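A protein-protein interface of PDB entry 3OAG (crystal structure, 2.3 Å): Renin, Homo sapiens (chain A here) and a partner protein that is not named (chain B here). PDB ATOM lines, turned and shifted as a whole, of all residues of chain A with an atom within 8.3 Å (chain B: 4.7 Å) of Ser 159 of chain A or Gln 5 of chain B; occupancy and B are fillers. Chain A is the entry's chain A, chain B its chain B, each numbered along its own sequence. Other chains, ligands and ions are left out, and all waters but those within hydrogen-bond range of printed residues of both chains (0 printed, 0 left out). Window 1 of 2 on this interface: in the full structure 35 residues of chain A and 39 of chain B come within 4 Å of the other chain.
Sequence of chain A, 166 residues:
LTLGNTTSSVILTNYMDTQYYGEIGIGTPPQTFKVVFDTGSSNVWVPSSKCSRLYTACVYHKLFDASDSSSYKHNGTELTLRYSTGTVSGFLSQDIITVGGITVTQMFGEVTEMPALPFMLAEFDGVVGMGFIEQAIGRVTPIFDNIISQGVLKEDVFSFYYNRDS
The backbone carbonyl oxygen of Asn 163 of chain A lies within hydrogen-bond range of the side-chain hydroxyl of Tyr 20 of chain A, 2.8 Å away. OH of Tyr 161 of chain A is in hydrogen-bond range of ND2 of Asn 163 of chain A (2.9 Å). NE2 of Gln 5 of chain B is in hydrogen-bond range of OD2 of Asp 12 of chain B (2.9 Å). The side-chain carboxylate (OD2) of Asp 12 of chain B sits at hydrogen-bond distance from a ring nitrogen (ND1) of His 15 of chain B, at 3.5 Å.
Of the 22 printed residues of chain A, 12 touch a printed residue of chain B. Printed residues of chain A that touch a printed residue of chain B: Ser 8, Ser 9, Val 10, Ile 11, Leu 12, Met 130, Val 157, Phe 158, Ser 159, Phe 160, Tyr 161 and Asn 163. Hydrophobic or aromatic side chains of chain A within 4 Å of the printed part of chain B: Val 10, Ile 11, Leu 12, Met 130, Val 157, Phe 158, Phe 160 and Tyr 161. Hydrophobic or aromatic side chains of chain B within 4 Å of the printed part of chain A: Leu 2, Ile 6, His 15 and Tyr 154. Along chain B the printed residues that touch a printed residue of chain A span positions 2 to 156. Among the printed residues, 33 pairs touch across the chains.
Printed residues of chain B within 4 Å of Leu 12 of chain A: Gly 4 (2.9 Å), Gln 5 (3.7 Å) and Ile 6 (3.9 Å). Ser 159 of chain A touches just these residues of chain B: Gln 5 (3.7 Å), Ile 6 (3.1 Å), Val 7 (2.8 Å), Gly 10 (2.7 Å), Ser 11 (3.5 Å), Tyr 154 (3.2 Å), Thr 155 (3.2 Å) and Glu 156 (3.5 Å). Of the printed residues of chain B, Asn 163 of chain A touches Leu 2. Of the printed residues of chain A, Leu 2 of chain B touches Ile 11, Tyr 161 and Asn 163. Gly 4 of chain B touches just these residues of chain A: Ile 11 (3.9 Å), Leu 12 (2.9 Å) and Tyr 161 (3.0 Å). Gln 5 of chain B touches just these residues of chain A: Val 10, Leu 12, Ser 159, Phe 160 and Tyr 161. Printed residues of chain A within 4 Å of Thr 155 of chain B: Ser 159 (3.2 Å) and Phe 160 (2.8 Å). The nearest printed residue of chain B that does not touch Ser 159 of chain A is Asp 12 of chain B (5.2 Å).
Among the printed residues, merely in contact across the chains: Phe 158 of chain A with Val 7 of chain B (3.0 Å), Tyr 161 of chain A with Gly 4 of chain B (3.0 Å), Ser 159 of chain A with Ile 6 of chain B (3.1 Å), Ser 9 of chain A with Ile 6 of chain B (3.2 Å), Ser 159 of chain A with Thr 155 of chain B (3.2 Å), Ser 159 of chain A with Tyr 154 of chain B (3.2 Å), Phe 160 of chain A with Gln 5 of chain B (3.5 Å), Ser 159 of chain A with Ser 11 of chain B (3.5 Å), Val 10 of chain A with Gln 5 of chain B (3.5 Å), Ser 8 of chain A with Val 7 of chain B (3.5 Å), Ser 159 of chain A with Glu 156 of chain B (3.5 Å), Ile 11 of chain A with Leu 2 of chain B (3.5 Å), Phe 160 of chain A with Tyr 154 of chain B (3.5 Å), Val 157 of chain A with Gly 10 of chain B (3.5 Å), Tyr 161 of chain A with Tyr 154 of chain B (3.6 Å), Phe 158 of chain A with Glu 156 of chain B (3.6 Å), Phe 160 of chain A with Ile 6 of chain B (3.7 Å), Leu 12 of chain A with Gln 5 of chain B (3.7 Å), Val 157 of chain A with Glu 156 of chain B (3.7 Å), Ser 159 of chain A with Gln 5 of chain B (3.7 Å), Tyr 161 of chain A with His 15 of chain B (3.8 Å), Met 130 of chain A with Ile 6 of chain B (3.8 Å), Ile 11 of chain A with Gly 4 of chain B (3.9 Å), Leu 12 of chain A with Ile 6 of chain B (3.9 Å), Ser 8 of chain A with Ile 6 of chain B (3.9 Å) and Tyr 161 of chain A with Leu 2 of chain B (3.9 Å).
The backbone carbonyl oxygen (O) of Ile 6 of chain B is in hydrogen-bond range of the backbone NH (N) of Val 10 of chain A. The backbone NH (N) of Leu 12 of chain A lies within hydrogen-bond range of the backbone carbonyl oxygen (O) of Gly 4 of chain B, 2.9 Å away. The backbone NH (N) of Ser 159 of chain A is in hydrogen-bond range of the backbone carbonyl oxygen (O) of Val 7 of chain B (2.8 Å). The backbone carbonyl oxygen of Gly 10 of chain B lies within hydrogen-bond range of the side-chain hydroxyl of Ser 159 of chain A, 2.7 Å away. N of Phe 160 of chain A is in hydrogen-bond range of O of Thr 155 of chain B. N of Tyr 161 of chain A sits at hydrogen-bond distance from O of Gln 5 of chain B (2.6 Å). The side-chain amide nitrogen (ND2) of Asn 163 of chain A lies within hydrogen-bond range of the backbone carbonyl oxygen (O) of Leu 2 of chain B, at 2.8 Å.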
ATOM      1  N   SER A   8      -6.620  17.520  29.997  1.00  0.00           N
ATOM      2  CA  SER A   8      -6.835  18.196  31.276  1.00  0.00           C
ATOM      3  C   SER A   8      -7.126  19.674  31.037  1.00  0.00           C
ATOM      4  O   SER A   8      -6.395  20.364  30.320  1.00  0.00           O
ATOM      5  CB  SER A   8      -5.622  18.021  32.193  1.00  0.00           C
ATOM      6  OG  SER A   8      -5.785  18.728  33.411  1.00  0.00           O
ATOM      7  N   SER A   9      -8.206  20.157  31.630  1.00  0.00           N
ATOM      8  CA  SER A   9      -8.623  21.525  31.389  1.00  0.00           C
ATOM      9  C   SER A   9      -8.550  22.385  32.648  1.00  0.00           C
ATOM     10  O   SER A   9      -8.537  21.871  33.769  1.00  0.00           O
ATOM     11  CB  SER A   9     -10.022  21.546  30.795  1.00  0.00           C
ATOM     12  OG  SER A   9     -10.982  21.334  31.803  1.00  0.00           O
ATOM     13  N   VAL A  10      -8.478  23.696  32.440  1.00  0.00           N
ATOM     14  CA  VAL A  10      -8.396  24.669  33.513  1.00  0.00           C
ATOM     15  C   VAL A  10      -9.348  25.797  33.162  1.00  0.00           C
ATOM     16  O   VAL A  10      -9.228  26.395  32.105  1.00  0.00           O
ATOM     17  CB  VAL A  10      -6.937  25.238  33.666  1.00  0.00           C
ATOM     18  CG1 VAL A  10      -6.845  26.270  34.796  1.00  0.00           C
ATOM     19  CG2 VAL A  10      -5.929  24.119  33.873  1.00  0.00           C
ATOM     20  N   ILE A  11     -10.308  26.067  34.034  1.00  0.00           N
ATOM     21  CA  ILE A  11     -11.231  27.174  33.819  1.00  0.00           C
ATOM     22  C   ILE A  11     -10.468  28.483  34.046  1.00  0.00           C
ATOM     23  O   ILE A  11      -9.675  28.601  34.989  1.00  0.00           O
ATOM     24  CB  ILE A  11     -12.483  27.104  34.747  1.00  0.00           C
ATOM     25  CG1 ILE A  11     -13.241  25.786  34.568  1.00  0.00           C
ATOM     26  CG2 ILE A  11     -13.426  28.269  34.503  1.00  0.00           C
ATOM     27  CD1 ILE A  11     -13.974  25.648  33.234  1.00  0.00           C
ATOM     28  N   LEU A  12     -10.694  29.449  33.162  1.00  0.00           N
ATOM     29  CA  LEU A  12     -10.079  30.745  33.290  1.00  0.00           C
ATOM     30  C   LEU A  12     -11.108  31.787  33.665  1.00  0.00           C
ATOM     31  O   LEU A  12     -12.287  31.669  33.331  1.00  0.00           O
ATOM     32  CB  LEU A  12      -9.375  31.155  31.997  1.00  0.00           C
ATOM     33  CG  LEU A  12      -8.299  30.230  31.449  1.00  0.00           C
ATOM     34  CD1 LEU A  12      -7.789  30.758  30.111  1.00  0.00           C
ATOM     35  CD2 LEU A  12      -7.154  30.043  32.448  1.00  0.00           C
ATOM     36  N   THR A  13     -10.637  32.793  34.392  1.00  0.00           N
ATOM     37  CA  THR A  13     -11.400  33.987  34.677  1.00  0.00           C
ATOM     38  C   THR A  13     -10.934  35.072  33.720  1.00  0.00           C
ATOM     39  O   THR A  13      -9.729  35.261  33.521  1.00  0.00           O
ATOM     40  CB  THR A  13     -11.151  34.440  36.115  1.00  0.00           C
ATOM     41  OG1 THR A  13     -11.610  33.416  36.987  1.00  0.00           O
ATOM     42  CG2 THR A  13     -11.878  35.758  36.438  1.00  0.00           C
ATOM     43  N   ASN A  14     -11.899  35.759  33.123  1.00  0.00           N
ATOM     44  CA  ASN A  14     -11.652  36.933  32.296  1.00  0.00           C
ATOM     45  C   ASN A  14     -11.819  38.194  33.137  1.00  0.00           C
ATOM     46  O   ASN A  14     -12.923  38.512  33.561  1.00  0.00           O
ATOM     47  CB  ASN A  14     -12.646  36.953  31.135  1.00  0.00           C
ATOM     48  CG  ASN A  14     -12.573  38.226  30.301  1.00  0.00           C
ATOM     49  OD1 ASN A  14     -11.778  39.120  30.564  1.00  0.00           O
ATOM     50  ND2 ASN A  14     -13.407  38.301  29.280  1.00  0.00           N
ATOM     51  N   TYR A  20      -6.481  37.051  31.495  1.00  0.00           N
ATOM     52  CA  TYR A  20      -7.084  35.730  31.589  1.00  0.00           C
ATOM     53  C   TYR A  20      -6.229  34.830  32.476  1.00  0.00           C
ATOM     54  O   TYR A  20      -5.045  34.618  32.203  1.00  0.00           O
ATOM     55  CB  TYR A  20      -7.288  35.114  30.204  1.00  0.00           C
ATOM     56  CG  TYR A  20      -8.274  35.872  29.329  1.00  0.00           C
ATOM     57  CD1 TYR A  20      -9.577  35.405  29.158  1.00  0.00           C
ATOM     58  CD2 TYR A  20      -7.895  37.059  28.672  1.00  0.00           C
ATOM     59  CE1 TYR A  20     -10.481  36.101  28.372  1.00  0.00           C
ATOM     60  CE2 TYR A  20      -8.791  37.762  27.868  1.00  0.00           C
ATOM     61  CZ  TYR A  20     -10.084  37.280  27.723  1.00  0.00           C
ATOM     62  OH  TYR A  20     -10.981  37.968  26.941  1.00  0.00           O
ATOM     63  N   TYR A  21      -6.839  34.288  33.524  1.00  0.00           N
ATOM     64  CA  TYR A  21      -6.109  33.500  34.528  1.00  0.00           C
ATOM     65  C   TYR A  21      -6.950  32.396  35.132  1.00  0.00           C
ATOM     66  O   TYR A  21      -8.175  32.542  35.255  1.00  0.00           O
ATOM     67  CB  TYR A  21      -5.571  34.397  35.665  1.00  0.00           C
ATOM     68  CG  TYR A  21      -6.612  35.271  36.336  1.00  0.00           C
ATOM     69  CD1 TYR A  21      -6.758  36.609  35.969  1.00  0.00           C
ATOM     70  CD2 TYR A  21      -7.446  34.774  37.335  1.00  0.00           C
ATOM     71  CE1 TYR A  21      -7.704  37.423  36.554  1.00  0.00           C
ATOM     72  CE2 TYR A  21      -8.412  35.597  37.947  1.00  0.00           C
ATOM     73  CZ  TYR A  21      -8.528  36.922  37.542  1.00  0.00           C
ATOM     74  OH  TYR A  21      -9.464  37.763  38.120  1.00  0.00           O
ATOM     75  N   PHE A  37      -1.553  31.839  31.824  1.00  0.00           N
ATOM     76  CA  PHE A  37      -0.817  30.837  31.056  1.00  0.00           C
ATOM     77  C   PHE A  37      -0.313  31.505  29.773  1.00  0.00           C
ATOM     78  O   PHE A  37      -1.098  31.837  28.877  1.00  0.00           O
ATOM     79  CB  PHE A  37      -1.686  29.616  30.791  1.00  0.00           C
ATOM     80  CG  PHE A  37      -2.138  28.899  32.063  1.00  0.00           C
ATOM     81  CD1 PHE A  37      -3.308  29.287  32.727  1.00  0.00           C
ATOM     82  CD2 PHE A  37      -1.400  27.834  32.579  1.00  0.00           C
ATOM     83  CE1 PHE A  37      -3.730  28.629  33.890  1.00  0.00           C
ATOM     84  CE2 PHE A  37      -1.805  27.175  33.741  1.00  0.00           C
ATOM     85  CZ  PHE A  37      -2.981  27.568  34.398  1.00  0.00           C
ATOM     86  N   THR A  39       2.068  31.972  26.530  1.00  0.00           N
ATOM     87  CA  THR A  39       2.912  31.434  25.447  1.00  0.00           C
ATOM     88  C   THR A  39       4.077  32.373  25.048  1.00  0.00           C
ATOM     89  O   THR A  39       4.951  32.007  24.255  1.00  0.00           O
ATOM     90  CB  THR A  39       2.080  31.033  24.226  1.00  0.00           C
ATOM     91  OG1 THR A  39       1.370  32.174  23.743  1.00  0.00           O
ATOM     92  CG2 THR A  39       1.077  29.935  24.602  1.00  0.00           C
ATOM     93  N   MET A 130       4.459  29.056  28.879  1.00  0.00           N
ATOM     94  CA  MET A 130       4.138  27.886  28.068  1.00  0.00           C
ATOM     95  C   MET A 130       4.993  27.845  26.822  1.00  0.00           C
ATOM     96  O   MET A 130       4.710  27.091  25.889  1.00  0.00           O
ATOM     97  CB  MET A 130       2.655  27.859  27.707  1.00  0.00           C
ATOM     98  CG  MET A 130       1.721  27.895  28.896  1.00  0.00           C
ATOM     99  SD  MET A 130       1.587  26.327  29.770  1.00  0.00           S
ATOM    100  CE  MET A 130       0.586  25.401  28.603  1.00  0.00           C
ATOM    101  N   PHE A 144       5.489  22.601  30.546  1.00  0.00           N
ATOM    102  CA  PHE A 144       4.844  21.751  29.559  1.00  0.00           C
ATOM    103  C   PHE A 144       5.783  20.678  29.048  1.00  0.00           C
ATOM    104  O   PHE A 144       5.326  19.628  28.601  1.00  0.00           O
ATOM    105  CB  PHE A 144       4.186  22.524  28.404  1.00  0.00           C
ATOM    106  CG  PHE A 144       3.148  21.707  27.669  1.00  0.00           C
ATOM    107  CD1 PHE A 144       1.989  21.278  28.328  1.00  0.00           C
ATOM    108  CD2 PHE A 144       3.352  21.318  26.349  1.00  0.00           C
ATOM    109  CE1 PHE A 144       1.029  20.506  27.668  1.00  0.00           C
ATOM    110  CE2 PHE A 144       2.401  20.536  25.669  1.00  0.00           C
ATOM    111  CZ  PHE A 144       1.235  20.136  26.321  1.00  0.00           C
ATOM    112  N   GLU A 155      -2.416  14.168  23.363  1.00  0.00           N
ATOM    113  CA  GLU A 155      -1.573  14.784  22.341  1.00  0.00           C
ATOM    114  C   GLU A 155      -0.646  15.811  22.985  1.00  0.00           C
ATOM    115  O   GLU A 155      -0.989  16.383  24.018  1.00  0.00           O
ATOM    116  CB  GLU A 155      -2.437  15.442  21.259  1.00  0.00           C
ATOM    117  CG  GLU A 155      -3.177  14.469  20.333  1.00  0.00           C
ATOM    118  CD  GLU A 155      -4.320  15.123  19.531  1.00  0.00           C
ATOM    119  OE1 GLU A 155      -4.447  16.374  19.524  1.00  0.00           O
ATOM    120  OE2 GLU A 155      -5.105  14.370  18.902  1.00  0.00           O
ATOM    121  N   ASP A 156       0.526  16.037  22.385  1.00  0.00           N
ATOM    122  CA  ASP A 156       1.471  17.058  22.868  1.00  0.00           C
ATOM    123  C   ASP A 156       1.050  18.456  22.384  1.00  0.00           C
ATOM    124  O   ASP A 156       1.774  19.137  21.640  1.00  0.00           O
ATOM    125  CB  ASP A 156       2.900  16.748  22.429  1.00  0.00           C
ATOM    126  CG  ASP A 156       3.487  15.497  23.102  1.00  0.00           C
ATOM    127  OD1 ASP A 156       2.895  14.947  24.067  1.00  0.00           O
ATOM    128  OD2 ASP A 156       4.569  15.067  22.648  1.00  0.00           O
ATOM    129  N   VAL A 157      -0.147  18.855  22.801  1.00  0.00           N
ATOM    130  CA  VAL A 157      -0.735  20.132  22.413  1.00  0.00           C
ATOM    131  C   VAL A 157      -1.428  20.732  23.614  1.00  0.00           C
ATOM    132  O   VAL A 157      -1.733  20.037  24.571  1.00  0.00           O
ATOM    133  CB  VAL A 157      -1.791  19.981  21.272  1.00  0.00           C
ATOM    134  CG1 VAL A 157      -1.165  19.373  20.017  1.00  0.00           C
ATOM    135  CG2 VAL A 157      -2.998  19.142  21.738  1.00  0.00           C
ATOM    136  N   PHE A 158      -1.658  22.032  23.560  1.00  0.00           N
ATOM    137  CA  PHE A 158      -2.544  22.698  24.499  1.00  0.00           C
ATOM    138  C   PHE A 158      -3.266  23.799  23.742  1.00  0.00           C
ATOM    139  O   PHE A 158      -2.743  24.342  22.766  1.00  0.00           O
ATOM    140  CB  PHE A 158      -1.785  23.244  25.719  1.00  0.00           C
ATOM    141  CG  PHE A 158      -0.657  24.164  25.377  1.00  0.00           C
ATOM    142  CD1 PHE A 158      -0.878  25.526  25.227  1.00  0.00           C
ATOM    143  CD2 PHE A 158       0.628  23.668  25.182  1.00  0.00           C
ATOM    144  CE1 PHE A 158       0.169  26.381  24.921  1.00  0.00           C
ATOM    145  CE2 PHE A 158       1.688  24.518  24.868  1.00  0.00           C
ATOM    146  CZ  PHE A 158       1.457  25.876  24.739  1.00  0.00           C
ATOM    147  N   SER A 159      -4.465  24.120  24.199  1.00  0.00           N
ATOM    148  CA  SER A 159      -5.340  25.012  23.474  1.00  0.00           C
ATOM    149  C   SER A 159      -5.913  26.070  24.387  1.00  0.00           C
ATOM    150  O   SER A 159      -6.125  25.824  25.573  1.00  0.00           O
ATOM    151  CB  SER A 159      -6.474  24.199  22.848  1.00  0.00           C
ATOM    152  OG  SER A 159      -5.938  23.192  22.007  1.00  0.00           O
ATOM    153  N   PHE A 160      -6.193  27.236  23.812  1.00  0.00           N
ATOM    154  CA  PHE A 160      -6.761  28.363  24.548  1.00  0.00           C
ATOM    155  C   PHE A 160      -8.121  28.782  24.008  1.00  0.00           C
ATOM    156  O   PHE A 160      -8.276  29.006  22.814  1.00  0.00           O
ATOM    157  CB  PHE A 160      -5.811  29.569  24.477  1.00  0.00           C
ATOM    158  CG  PHE A 160      -4.641  29.493  25.429  1.00  0.00           C
ATOM    159  CD1 PHE A 160      -3.551  28.661  25.157  1.00  0.00           C
ATOM    160  CD2 PHE A 160      -4.624  30.264  26.596  1.00  0.00           C
ATOM    161  CE1 PHE A 160      -2.459  28.595  26.043  1.00  0.00           C
ATOM    162  CE2 PHE A 160      -3.539  30.213  27.485  1.00  0.00           C
ATOM    163  CZ  PHE A 160      -2.453  29.388  27.207  1.00  0.00           C
ATOM    164  N   TYR A 161      -9.098  28.886  24.900  1.00  0.00           N
ATOM    165  CA  TYR A 161     -10.319  29.620  24.626  1.00  0.00           C
ATOM    166  C   TYR A 161     -10.372  30.820  25.556  1.00  0.00           C
ATOM    167  O   TYR A 161     -10.210  30.686  26.776  1.00  0.00           O
ATOM    168  CB  TYR A 161     -11.557  28.737  24.822  1.00  0.00           C
ATOM    169  CG  TYR A 161     -12.870  29.491  24.864  1.00  0.00           C
ATOM    170  CD1 TYR A 161     -13.342  30.168  23.751  1.00  0.00           C
ATOM    171  CD2 TYR A 161     -13.647  29.513  26.022  1.00  0.00           C
ATOM    172  CE1 TYR A 161     -14.559  30.867  23.787  1.00  0.00           C
ATOM    173  CE2 TYR A 161     -14.863  30.200  26.072  1.00  0.00           C
ATOM    174  CZ  TYR A 161     -15.312  30.873  24.955  1.00  0.00           C
ATOM    175  OH  TYR A 161     -16.516  31.556  24.990  1.00  0.00           O
ATOM    176  N   TYR A 162     -10.601  31.988  24.969  1.00  0.00           N
ATOM    177  CA  TYR A 162     -10.822  33.221  25.716  1.00  0.00           C
ATOM    178  C   TYR A 162     -12.190  33.807  25.323  1.00  0.00           C
ATOM    179  O   TYR A 162     -12.398  34.132  24.159  1.00  0.00           O
ATOM    180  CB  TYR A 162      -9.741  34.258  25.363  1.00  0.00           C
ATOM    181  CG  TYR A 162      -8.361  34.107  25.997  1.00  0.00           C
ATOM    182  CD1 TYR A 162      -8.079  33.115  26.952  1.00  0.00           C
ATOM    183  CD2 TYR A 162      -7.351  34.989  25.653  1.00  0.00           C
ATOM    184  CE1 TYR A 162      -6.824  33.005  27.525  1.00  0.00           C
ATOM    185  CE2 TYR A 162      -6.090  34.897  26.213  1.00  0.00           C
ATOM    186  CZ  TYR A 162      -5.825  33.903  27.149  1.00  0.00           C
ATOM    187  OH  TYR A 162      -4.563  33.840  27.702  1.00  0.00           O
ATOM    188  N   ASN A 163     -13.096  33.964  26.287  1.00  0.00           N
ATOM    189  CA  ASN A 163     -14.432  34.554  26.051  1.00  0.00           C
ATOM    190  C   ASN A 163     -14.375  36.078  26.008  1.00  0.00           C
ATOM    191  O   ASN A 163     -13.336  36.682  26.271  1.00  0.00           O
ATOM    192  CB  ASN A 163     -15.406  34.132  27.162  1.00  0.00           C
ATOM    193  CG  ASN A 163     -16.862  33.966  26.671  1.00  0.00           C
ATOM    194  OD1 ASN A 163     -17.354  34.701  25.798  1.00  0.00           O
ATOM    195  ND2 ASN A 163     -17.558  32.990  27.252  1.00  0.00           N
ATOM    196  N   LEU B   2     -18.426  31.736  31.640  1.00  0.00           N
ATOM    197  CA  LEU B   2     -17.114  31.092  31.455  1.00  0.00           C
ATOM    198  C   LEU B   2     -16.129  32.065  30.815  1.00  0.00           C
ATOM    199  O   LEU B   2     -16.255  32.387  29.635  1.00  0.00           O
ATOM    200  CB  LEU B   2     -17.216  29.825  30.587  1.00  0.00           C
ATOM    201  CG  LEU B   2     -15.871  29.131  30.302  1.00  0.00           C
ATOM    202  CD1 LEU B   2     -15.330  28.471  31.555  1.00  0.00           C
ATOM    203  CD2 LEU B   2     -15.946  28.118  29.180  1.00  0.00           C
ATOM    204  N   GLY B   4     -12.966  31.729  30.076  1.00  0.00           N
ATOM    205  CA  GLY B   4     -12.016  31.114  29.169  1.00  0.00           C
ATOM    206  C   GLY B   4     -11.656  29.719  29.624  1.00  0.00           C
ATOM    207  O   GLY B   4     -12.132  29.249  30.658  1.00  0.00           O
ATOM    208  N   GLN B   5     -10.804  29.063  28.843  1.00  0.00           N
ATOM    209  CA  GLN B   5     -10.437  27.685  29.088  1.00  0.00           C
ATOM    210  C   GLN B   5      -9.140  27.339  28.374  1.00  0.00           C
ATOM    211  O   GLN B   5      -8.942  27.681  27.192  1.00  0.00           O
ATOM    212  CB  GLN B   5     -11.548  26.757  28.605  1.00  0.00           C
ATOM    213  CG  GLN B   5     -11.290  25.282  28.846  1.00  0.00           C
ATOM    214  CD  GLN B   5     -12.154  24.404  27.964  1.00  0.00           C
ATOM    215  OE1 GLN B   5     -12.204  24.586  26.746  1.00  0.00           O
ATOM    216  NE2 GLN B   5     -12.835  23.447  28.569  1.00  0.00           N
ATOM    217  N   ILE B   6      -8.250  26.679  29.111  1.00  0.00           N
ATOM    218  CA  ILE B   6      -7.079  26.055  28.526  1.00  0.00           C
ATOM    219  C   ILE B   6      -7.210  24.540  28.658  1.00  0.00           C
ATOM    220  O   ILE B   6      -7.553  24.022  29.727  1.00  0.00           O
ATOM    221  CB  ILE B   6      -5.730  26.604  29.122  1.00  0.00           C
ATOM    222  CG1 ILE B   6      -4.585  25.601  28.930  1.00  0.00           C
ATOM    223  CG2 ILE B   6      -5.861  26.917  30.601  1.00  0.00           C
ATOM    224  CD1 ILE B   6      -3.153  26.241  28.960  1.00  0.00           C
ATOM    225  N   VAL B   7      -6.973  23.849  27.549  1.00  0.00           N
ATOM    226  CA  VAL B   7      -6.931  22.395  27.520  1.00  0.00           C
ATOM    227  C   VAL B   7      -5.487  21.950  27.329  1.00  0.00           C
ATOM    228  O   VAL B   7      -4.771  22.491  26.484  1.00  0.00           O
ATOM    229  CB  VAL B   7      -7.809  21.817  26.388  1.00  0.00           C
ATOM    230  CG1 VAL B   7      -7.725  20.288  26.371  1.00  0.00           C
ATOM    231  CG2 VAL B   7      -9.244  22.261  26.548  1.00  0.00           C
ATOM    232  N   GLY B  10      -5.194  18.382  24.403  1.00  0.00           N
ATOM    233  CA  GLY B  10      -6.186  18.434  23.339  1.00  0.00           C
ATOM    234  C   GLY B  10      -6.775  19.807  23.064  1.00  0.00           C
ATOM    235  O   GLY B  10      -6.151  20.859  23.336  1.00  0.00           O
ATOM    236  N   SER B  11      -7.987  19.780  22.508  1.00  0.00           N
ATOM    237  CA  SER B  11      -8.798  20.975  22.291  1.00  0.00           C
ATOM    238  C   SER B  11     -10.230  20.645  22.683  1.00  0.00           C
ATOM    239  O   SER B  11     -10.565  19.479  22.905  1.00  0.00           O
ATOM    240  CB  SER B  11      -8.717  21.434  20.834  1.00  0.00           C
ATOM    241  OG  SER B  11      -9.298  20.468  19.966  1.00  0.00           O
ATOM    242  N   ASP B  12     -11.067  21.668  22.792  1.00  0.00           N
ATOM    243  CA  ASP B  12     -12.452  21.480  23.216  1.00  0.00           C
ATOM    244  C   ASP B  12     -13.388  21.976  22.112  1.00  0.00           C
ATOM    245  O   ASP B  12     -13.586  23.187  21.963  1.00  0.00           O
ATOM    246  CB  ASP B  12     -12.690  22.202  24.545  1.00  0.00           C
ATOM    247  CG  ASP B  12     -14.057  21.910  25.157  1.00  0.00           C
ATOM    248  OD1 ASP B  12     -14.928  21.292  24.491  1.00  0.00           O
ATOM    249  OD2 ASP B  12     -14.258  22.319  26.327  1.00  0.00           O
ATOM    250  N   HIS B  15     -16.091  24.816  21.897  1.00  0.00           N
ATOM    251  CA  HIS B  15     -15.658  26.220  21.948  1.00  0.00           C
ATOM    252  C   HIS B  15     -15.067  26.808  20.659  1.00  0.00           C
ATOM    253  O   HIS B  15     -14.721  27.996  20.609  1.00  0.00           O
ATOM    254  CB  HIS B  15     -14.712  26.436  23.125  1.00  0.00           C
ATOM    255  CG  HIS B  15     -15.402  26.395  24.449  1.00  0.00           C
ATOM    256  ND1 HIS B  15     -14.975  25.597  25.487  1.00  0.00           N
ATOM    257  CD2 HIS B  15     -16.514  27.027  24.890  1.00  0.00           C
ATOM    258  CE1 HIS B  15     -15.782  25.756  26.520  1.00  0.00           C
ATOM    259  NE2 HIS B  15     -16.728  26.615  26.181  1.00  0.00           N
ATOM    260  N   TYR B 154      -9.955  30.589  18.410  1.00  0.00           N
ATOM    261  CA  TYR B 154      -9.505  29.496  19.256  1.00  0.00           C
ATOM    262  C   TYR B 154      -8.129  29.071  18.749  1.00  0.00           C
ATOM    263  O   TYR B 154      -7.937  28.874  17.539  1.00  0.00           O
ATOM    264  CB  TYR B 154     -10.489  28.327  19.161  1.00  0.00           C
ATOM    265  CG  TYR B 154     -10.275  27.225  20.181  1.00  0.00           C
ATOM    266  CD1 TYR B 154      -9.384  26.171  19.931  1.00  0.00           C
ATOM    267  CD2 TYR B 154     -10.966  27.230  21.388  1.00  0.00           C
ATOM    268  CE1 TYR B 154      -9.201  25.151  20.865  1.00  0.00           C
ATOM    269  CE2 TYR B 154     -10.781  26.228  22.333  1.00  0.00           C
ATOM    270  CZ  TYR B 154      -9.899  25.195  22.066  1.00  0.00           C
ATOM    271  OH  TYR B 154      -9.718  24.216  23.005  1.00  0.00           O
ATOM    272  N   THR B 155      -7.170  28.967  19.667  1.00  0.00           N
ATOM    273  CA  THR B 155      -5.785  28.696  19.282  1.00  0.00           C
ATOM    274  C   THR B 155      -5.229  27.415  19.905  1.00  0.00           C
ATOM    275  O   THR B 155      -5.334  27.198  21.108  1.00  0.00           O
ATOM    276  CB  THR B 155      -4.866  29.891  19.594  1.00  0.00           C
ATOM    277  OG1 THR B 155      -5.417  31.080  19.017  1.00  0.00           O
ATOM    278  CG2 THR B 155      -3.516  29.668  19.001  1.00  0.00           C
ATOM    279  N   GLU B 156      -4.647  26.574  19.056  1.00  0.00           N
ATOM    280  CA  GLU B 156      -3.969  25.355  19.481  1.00  0.00           C
ATOM    281  C   GLU B 156      -2.462  25.473  19.298  1.00  0.00           C
ATOM    282  O   GLU B 156      -1.993  25.822  18.224  1.00  0.00           O
ATOM    283  CB  GLU B 156      -4.477  24.156  18.689  1.00  0.00           C
ATOM    284  CG  GLU B 156      -3.888  22.855  19.184  1.00  0.00           C
ATOM    285  CD  GLU B 156      -4.360  21.662  18.395  1.00  0.00           C
ATOM    286  OE1 GLU B 156      -3.528  21.060  17.676  1.00  0.00           O
ATOM    287  OE2 GLU B 156      -5.561  21.333  18.491  1.00  0.00           O
